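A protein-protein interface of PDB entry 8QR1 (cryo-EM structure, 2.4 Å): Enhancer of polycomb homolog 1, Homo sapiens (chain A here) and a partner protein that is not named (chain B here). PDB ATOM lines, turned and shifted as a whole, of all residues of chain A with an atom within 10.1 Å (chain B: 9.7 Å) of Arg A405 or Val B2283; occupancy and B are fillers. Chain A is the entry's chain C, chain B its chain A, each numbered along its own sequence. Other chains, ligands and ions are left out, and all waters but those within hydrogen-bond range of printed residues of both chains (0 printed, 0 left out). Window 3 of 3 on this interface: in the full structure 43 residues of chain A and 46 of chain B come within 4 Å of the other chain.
Of the 8 printed residues of chain B, 7 touch a printed residue of chain A. Hydrophobic or aromatic side chains of chain B that line the printed part of chain A: Leu B799, Pro B800, Leu B802, Pro B2281 and Val B2283. Of the 15 printed residues of chain A, 8 touch a printed residue of chain B. Hydrophobic or aromatic side chains of chain A that line the printed part of chain B: Phe A404 and Tyr A412.
N of Lys A407 sits at hydrogen-bond distance from OH of Tyr A412, 3.3 Å away.
Asp A397 touches none of the printed residues of chain B. Pro A398 touches none of the printed residues of chain B. Printed residues of chain B within 4 Å of Phe A402: Leu B799. Ala A403 touches one residue of chain B. Of the printed residues of chain B, Arg A405 touches Val B2283 (2.8 Å). Printed residues of chain B within 4 Å of Cys A410: Leu B802. Of the printed residues of chain A, Leu B799 touches Phe A402, Ala A403 and Phe A404. Printed residues of chain A within 4 Å of Leu B802: Cys A410 (3.7 Å) and Tyr A412 (3.6 Å). Of the printed residues of chain A, Pro B2281 touches Phe A404 and Arg A406. Pro B2282 touches just one residue of chain A: Arg A406. Of chain A, only Arg A405, Arg A406 and Ala A408 come within 4 Å of Val B2283. The nearest residue of chain A that does not touch Val B2283 is Lys A407 (4.4 Å). The nearest printed residue of chain B that does not touch Tyr A412 is Leu B799 (7.0 Å).
The backbone carbonyl oxygen (O) of Pro B2281 sits at hydrogen-bond distance from the guanidinium group (NH1) of Arg A406 (3.2 Å). The backbone carbonyl oxygen (O) of Pro B2282 is in hydrogen-bond range of the guanidinium group (NH1) of Arg A406 (3.3 Å). O of Val B2283 is in hydrogen-bond range of NH2 of Arg A405 (2.8 Å).
Among the printed residues, pairs that only touch across the chains: Phe A402 with Leu B799 (3.3 Å), Ala A403 with Leu B799 (3.9 Å), Phe A404 with Leu B799 (3.5 Å), Phe A404 with Pro B800 (3.7 Å), Phe A404 with Pro B2281 (3.4 Å), Arg A406 with Val B2283 (3.0 Å), Ala A408 with Val B2283 (3.8 Å), Cys A410 with Leu B802 (3.7 Å), Tyr A412 with Pro B800 (3.99 Å), Tyr A412 with Leu B802 (3.6 Å) and Tyr A412 with Lys B2279 (3.9 Å).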
ATOM      1  N   ASP A 397      -8.652 -24.148  -2.008  1.00  0.00           N
ATOM      2  CA  ASP A 397      -8.479 -24.726  -3.372  1.00  0.00           C
ATOM      3  C   ASP A 397      -8.936 -23.713  -4.440  1.00  0.00           C
ATOM      4  O   ASP A 397     -10.110 -23.709  -4.815  1.00  0.00           O
ATOM      5  CB  ASP A 397      -9.256 -26.039  -3.492  1.00  0.00           C
ATOM      6  CG  ASP A 397      -9.078 -26.931  -2.279  1.00  0.00           C
ATOM      7  OD1 ASP A 397      -8.785 -28.132  -2.461  1.00  0.00           O
ATOM      8  OD2 ASP A 397      -9.234 -26.434  -1.144  1.00  0.00           O
ATOM      9  N   PRO A 398      -8.033 -22.835  -4.909  1.00  0.00           N
ATOM     10  CA  PRO A 398      -8.461 -21.846  -5.917  1.00  0.00           C
ATOM     11  C   PRO A 398      -8.924 -22.461  -7.224  1.00  0.00           C
ATOM     12  O   PRO A 398      -9.951 -22.041  -7.770  1.00  0.00           O
ATOM     13  CB  PRO A 398      -7.205 -20.985  -6.118  1.00  0.00           C
ATOM     14  CG  PRO A 398      -6.399 -21.185  -4.906  1.00  0.00           C
ATOM     15  CD  PRO A 398      -6.636 -22.598  -4.502  1.00  0.00           C
ATOM     16  N   ASP A 399      -8.200 -23.459  -7.732  1.00  0.00           N
ATOM     17  CA  ASP A 399      -8.487 -24.078  -9.019  1.00  0.00           C
ATOM     18  C   ASP A 399      -9.368 -25.319  -8.900  1.00  0.00           C
ATOM     19  O   ASP A 399      -9.585 -26.007  -9.903  1.00  0.00           O
ATOM     20  CB  ASP A 399      -7.183 -24.430  -9.731  1.00  0.00           C
ATOM     21  CG  ASP A 399      -6.328 -23.215 -10.025  1.00  0.00           C
ATOM     22  OD1 ASP A 399      -6.884 -22.100 -10.129  1.00  0.00           O
ATOM     23  OD2 ASP A 399      -5.097 -23.374 -10.156  1.00  0.00           O
ATOM     24  N   GLY A 400      -9.880 -25.626  -7.710  1.00  0.00           N
ATOM     25  CA  GLY A 400     -10.762 -26.754  -7.552  1.00  0.00           C
ATOM     26  C   GLY A 400     -10.006 -28.068  -7.633  1.00  0.00           C
ATOM     27  O   GLY A 400      -8.842 -28.146  -7.226  1.00  0.00           O
ATOM     28  N   PRO A 401     -10.639 -29.133  -8.141  1.00  0.00           N
ATOM     29  CA  PRO A 401      -9.893 -30.387  -8.339  1.00  0.00           C
ATOM     30  C   PRO A 401      -8.746 -30.274  -9.324  1.00  0.00           C
ATOM     31  O   PRO A 401      -7.807 -31.073  -9.244  1.00  0.00           O
ATOM     32  CB  PRO A 401     -10.962 -31.358  -8.855  1.00  0.00           C
ATOM     33  CG  PRO A 401     -12.239 -30.800  -8.398  1.00  0.00           C
ATOM     34  CD  PRO A 401     -12.073 -29.323  -8.423  1.00  0.00           C
ATOM     35  N   PHE A 402      -8.778 -29.301 -10.234  1.00  0.00           N
ATOM     36  CA  PHE A 402      -7.832 -29.213 -11.334  1.00  0.00           C
ATOM     37  C   PHE A 402      -6.606 -28.375 -10.993  1.00  0.00           C
ATOM     38  O   PHE A 402      -6.008 -27.767 -11.886  1.00  0.00           O
ATOM     39  CB  PHE A 402      -8.539 -28.654 -12.565  1.00  0.00           C
ATOM     40  CG  PHE A 402      -9.812 -29.368 -12.891  1.00  0.00           C
ATOM     41  CD1 PHE A 402      -9.786 -30.613 -13.485  1.00  0.00           C
ATOM     42  CD2 PHE A 402     -11.033 -28.808 -12.581  1.00  0.00           C
ATOM     43  CE1 PHE A 402     -10.952 -31.277 -13.776  1.00  0.00           C
ATOM     44  CE2 PHE A 402     -12.202 -29.472 -12.869  1.00  0.00           C
ATOM     45  CZ  PHE A 402     -12.161 -30.706 -13.468  1.00  0.00           C
ATOM     46  N   ALA A 403      -6.222 -28.328  -9.720  1.00  0.00           N
ATOM     47  CA  ALA A 403      -4.965 -27.703  -9.346  1.00  0.00           C
ATOM     48  C   ALA A 403      -3.797 -28.539  -9.847  1.00  0.00           C
ATOM     49  O   ALA A 403      -3.863 -29.771  -9.886  1.00  0.00           O
ATOM     50  CB  ALA A 403      -4.885 -27.541  -7.830  1.00  0.00           C
ATOM     51  N   PHE A 404      -2.719 -27.857 -10.231  1.00  0.00           N
ATOM     52  CA  PHE A 404      -1.541 -28.503 -10.808  1.00  0.00           C
ATOM     53  C   PHE A 404      -0.663 -29.011  -9.667  1.00  0.00           C
ATOM     54  O   PHE A 404       0.316 -28.384  -9.257  1.00  0.00           O
ATOM     55  CB  PHE A 404      -0.801 -27.523 -11.715  1.00  0.00           C
ATOM     56  CG  PHE A 404       0.454 -28.074 -12.372  1.00  0.00           C
ATOM     57  CD1 PHE A 404       0.607 -29.419 -12.674  1.00  0.00           C
ATOM     58  CD2 PHE A 404       1.483 -27.213 -12.698  1.00  0.00           C
ATOM     59  CE1 PHE A 404       1.755 -29.881 -13.267  1.00  0.00           C
ATOM     60  CE2 PHE A 404       2.631 -27.677 -13.293  1.00  0.00           C
ATOM     61  CZ  PHE A 404       2.765 -29.010 -13.579  1.00  0.00           C
ATOM     62  N   ARG A 405      -1.030 -30.185  -9.153  1.00  0.00           N
ATOM     63  CA  ARG A 405      -0.221 -30.885  -8.165  1.00  0.00           C
ATOM     64  C   ARG A 405       0.915 -31.608  -8.873  1.00  0.00           C
ATOM     65  O   ARG A 405       0.732 -32.709  -9.399  1.00  0.00           O
ATOM     66  CB  ARG A 405      -1.070 -31.889  -7.369  1.00  0.00           C
ATOM     67  CG  ARG A 405      -1.939 -31.368  -6.189  1.00  0.00           C
ATOM     68  CD  ARG A 405      -1.368 -30.200  -5.372  1.00  0.00           C
ATOM     69  NE  ARG A 405      -0.004 -30.450  -4.910  1.00  0.00           N
ATOM     70  CZ  ARG A 405       0.345 -31.330  -3.979  1.00  0.00           C
ATOM     71  NH1 ARG A 405      -0.551 -32.058  -3.328  1.00  0.00           N
ATOM     72  NH2 ARG A 405       1.634 -31.486  -3.689  1.00  0.00           N
ATOM     73  N   ARG A 406       2.089 -30.988  -8.888  1.00  0.00           N
ATOM     74  CA  ARG A 406       3.243 -31.562  -9.563  1.00  0.00           C
ATOM     75  C   ARG A 406       3.719 -32.812  -8.835  1.00  0.00           C
ATOM     76  O   ARG A 406       3.536 -32.951  -7.624  1.00  0.00           O
ATOM     77  CB  ARG A 406       4.357 -30.515  -9.636  1.00  0.00           C
ATOM     78  CG  ARG A 406       5.622 -30.928 -10.372  1.00  0.00           C
ATOM     79  CD  ARG A 406       6.643 -29.814 -10.326  1.00  0.00           C
ATOM     80  NE  ARG A 406       7.963 -30.246 -10.770  1.00  0.00           N
ATOM     81  CZ  ARG A 406       9.092 -29.572 -10.586  1.00  0.00           C
ATOM     82  NH1 ARG A 406       9.121 -28.413  -9.942  1.00  0.00           N
ATOM     83  NH2 ARG A 406      10.227 -30.071 -11.064  1.00  0.00           N
ATOM     84  N   LYS A 407       4.315 -33.729  -9.595  1.00  0.00           N
ATOM     85  CA  LYS A 407       4.940 -34.935  -9.073  1.00  0.00           C
ATOM     86  C   LYS A 407       6.424 -34.916  -9.409  1.00  0.00           C
ATOM     87  O   LYS A 407       6.825 -34.436 -10.473  1.00  0.00           O
ATOM     88  CB  LYS A 407       4.286 -36.193  -9.649  1.00  0.00           C
ATOM     89  CG  LYS A 407       4.886 -37.485  -9.125  1.00  0.00           C
ATOM     90  CD  LYS A 407       3.940 -38.669  -9.268  1.00  0.00           C
ATOM     91  CE  LYS A 407       2.881 -38.703  -8.176  1.00  0.00           C
ATOM     92  NZ  LYS A 407       2.154 -40.000  -8.153  1.00  0.00           N
ATOM     93  N   ALA A 408       7.234 -35.433  -8.489  1.00  0.00           N
ATOM     94  CA  ALA A 408       8.679 -35.364  -8.636  1.00  0.00           C
ATOM     95  C   ALA A 408       9.154 -36.224  -9.799  1.00  0.00           C
ATOM     96  O   ALA A 408       8.678 -37.344 -10.004  1.00  0.00           O
ATOM     97  CB  ALA A 408       9.356 -35.810  -7.343  1.00  0.00           C
ATOM     98  N   GLY A 409      10.106 -35.687 -10.563  1.00  0.00           N
ATOM     99  CA  GLY A 409      10.701 -36.390 -11.678  1.00  0.00           C
ATOM    100  C   GLY A 409       9.987 -36.229 -13.000  1.00  0.00           C
ATOM    101  O   GLY A 409      10.571 -36.545 -14.043  1.00  0.00           O
ATOM    102  N   CYS A 410       8.749 -35.742 -12.997  1.00  0.00           N
ATOM    103  CA  CYS A 410       7.982 -35.613 -14.224  1.00  0.00           C
ATOM    104  C   CYS A 410       8.328 -34.313 -14.945  1.00  0.00           C
ATOM    105  O   CYS A 410       8.842 -33.358 -14.354  1.00  0.00           O
ATOM    106  CB  CYS A 410       6.489 -35.653 -13.918  1.00  0.00           C
ATOM    107  SG  CYS A 410       5.940 -37.155 -13.093  1.00  0.00           S
ATOM    108  N   TYR A 412       6.566 -31.599 -18.073  1.00  0.00           N
ATOM    109  CA  TYR A 412       5.256 -31.157 -18.526  1.00  0.00           C
ATOM    110  C   TYR A 412       5.398 -30.196 -19.696  1.00  0.00           C
ATOM    111  O   TYR A 412       6.360 -29.427 -19.771  1.00  0.00           O
ATOM    112  CB  TYR A 412       4.489 -30.478 -17.391  1.00  0.00           C
ATOM    113  CG  TYR A 412       4.282 -31.345 -16.173  1.00  0.00           C
ATOM    114  CD1 TYR A 412       5.226 -31.389 -15.160  1.00  0.00           C
ATOM    115  CD2 TYR A 412       3.141 -32.113 -16.032  1.00  0.00           C
ATOM    116  CE1 TYR A 412       5.039 -32.176 -14.046  1.00  0.00           C
ATOM    117  CE2 TYR A 412       2.948 -32.903 -14.923  1.00  0.00           C
ATOM    118  CZ  TYR A 412       3.897 -32.930 -13.933  1.00  0.00           C
ATOM    119  OH  TYR A 412       3.700 -33.718 -12.827  1.00  0.00           O
ATOM    120  N   LEU B 799      -4.573 -27.351 -17.281  1.00  0.00           N
ATOM    121  CA  LEU B 799      -3.444 -28.113 -16.790  1.00  0.00           C
ATOM    122  C   LEU B 799      -2.497 -28.440 -17.948  1.00  0.00           C
ATOM    123  O   LEU B 799      -2.930 -28.512 -19.102  1.00  0.00           O
ATOM    124  CB  LEU B 799      -3.915 -29.405 -16.136  1.00  0.00           C
ATOM    125  CG  LEU B 799      -4.537 -29.313 -14.747  1.00  0.00           C
ATOM    126  CD1 LEU B 799      -5.262 -30.597 -14.449  1.00  0.00           C
ATOM    127  CD2 LEU B 799      -3.493 -29.042 -13.694  1.00  0.00           C
ATOM    128  N   PRO B 800      -1.206 -28.647 -17.675  1.00  0.00           N
ATOM    129  CA  PRO B 800      -0.286 -28.994 -18.760  1.00  0.00           C
ATOM    130  C   PRO B 800      -0.280 -30.484 -19.057  1.00  0.00           C
ATOM    131  O   PRO B 800      -0.733 -31.308 -18.258  1.00  0.00           O
ATOM    132  CB  PRO B 800       1.068 -28.531 -18.223  1.00  0.00           C
ATOM    133  CG  PRO B 800       0.959 -28.722 -16.792  1.00  0.00           C
ATOM    134  CD  PRO B 800      -0.463 -28.433 -16.420  1.00  0.00           C
ATOM    135  N   LEU B 802       1.351 -33.994 -19.396  1.00  0.00           N
ATOM    136  CA  LEU B 802       2.461 -34.781 -18.882  1.00  0.00           C
ATOM    137  C   LEU B 802       3.282 -35.349 -20.029  1.00  0.00           C
ATOM    138  O   LEU B 802       2.735 -35.886 -20.996  1.00  0.00           O
ATOM    139  CB  LEU B 802       1.930 -35.907 -17.997  1.00  0.00           C
ATOM    140  CG  LEU B 802       2.922 -36.855 -17.321  1.00  0.00           C
ATOM    141  CD1 LEU B 802       3.578 -36.173 -16.159  1.00  0.00           C
ATOM    142  CD2 LEU B 802       2.220 -38.101 -16.861  1.00  0.00           C
ATOM    143  N   LYS B2279       8.418 -23.864 -13.583  1.00  0.00           N
ATOM    144  CA  LYS B2279       7.251 -24.529 -13.016  1.00  0.00           C
ATOM    145  C   LYS B2279       6.981 -24.025 -11.606  1.00  0.00           C
ATOM    146  O   LYS B2279       7.807 -24.203 -10.704  1.00  0.00           O
ATOM    147  CB  LYS B2279       7.448 -26.048 -12.989  1.00  0.00           C
ATOM    148  CG  LYS B2279       6.814 -26.786 -14.156  1.00  0.00           C
ATOM    149  CD  LYS B2279       7.305 -28.229 -14.257  1.00  0.00           C
ATOM    150  CE  LYS B2279       8.722 -28.350 -14.816  1.00  0.00           C
ATOM    151  NZ  LYS B2279       8.845 -29.433 -15.830  1.00  0.00           N
ATOM    152  N   LEU B2280       5.828 -23.389 -11.418  1.00  0.00           N
ATOM    153  CA  LEU B2280       5.521 -22.772 -10.130  1.00  0.00           C
ATOM    154  C   LEU B2280       5.421 -23.759  -8.967  1.00  0.00           C
ATOM    155  O   LEU B2280       5.988 -23.454  -7.903  1.00  0.00           O
ATOM    156  CB  LEU B2280       4.233 -21.938 -10.242  1.00  0.00           C
ATOM    157  CG  LEU B2280       4.173 -20.688 -11.145  1.00  0.00           C
ATOM    158  CD1 LEU B2280       5.375 -19.764 -10.950  1.00  0.00           C
ATOM    159  CD2 LEU B2280       4.016 -21.040 -12.626  1.00  0.00           C
ATOM    160  N   PRO B2281       4.740 -24.905  -9.061  1.00  0.00           N
ATOM    161  CA  PRO B2281       4.638 -25.779  -7.887  1.00  0.00           C
ATOM    162  C   PRO B2281       5.984 -26.406  -7.559  1.00  0.00           C
ATOM    163  O   PRO B2281       6.699 -26.836  -8.477  1.00  0.00           O
ATOM    164  CB  PRO B2281       3.621 -26.848  -8.319  1.00  0.00           C
ATOM    165  CG  PRO B2281       2.952 -26.297  -9.509  1.00  0.00           C
ATOM    166  CD  PRO B2281       3.990 -25.489 -10.188  1.00  0.00           C
ATOM    167  N   PRO B2282       6.389 -26.479  -6.269  1.00  0.00           N
ATOM    168  CA  PRO B2282       7.603 -27.245  -5.959  1.00  0.00           C
ATOM    169  C   PRO B2282       7.423 -28.732  -6.216  1.00  0.00           C
ATOM    170  O   PRO B2282       8.258 -29.360  -6.873  1.00  0.00           O
ATOM    171  CB  PRO B2282       7.843 -26.950  -4.472  1.00  0.00           C
ATOM    172  CG  PRO B2282       7.132 -25.687  -4.215  1.00  0.00           C
ATOM    173  CD  PRO B2282       5.929 -25.727  -5.086  1.00  0.00           C
ATOM    174  N   VAL B2283       6.338 -29.304  -5.705  1.00  0.00           N
ATOM    175  CA  VAL B2283       6.065 -30.720  -5.895  1.00  0.00           C
ATOM    176  C   VAL B2283       4.593 -30.997  -5.611  1.00  0.00           C
ATOM    177  O   VAL B2283       4.004 -30.414  -4.701  1.00  0.00           O
ATOM    178  CB  VAL B2283       6.977 -31.593  -5.006  1.00  0.00           C
ATOM    179  CG1 VAL B2283       6.559 -31.504  -3.538  1.00  0.00           C
ATOM    180  CG2 VAL B2283       6.987 -33.034  -5.493  1.00  0.00           C
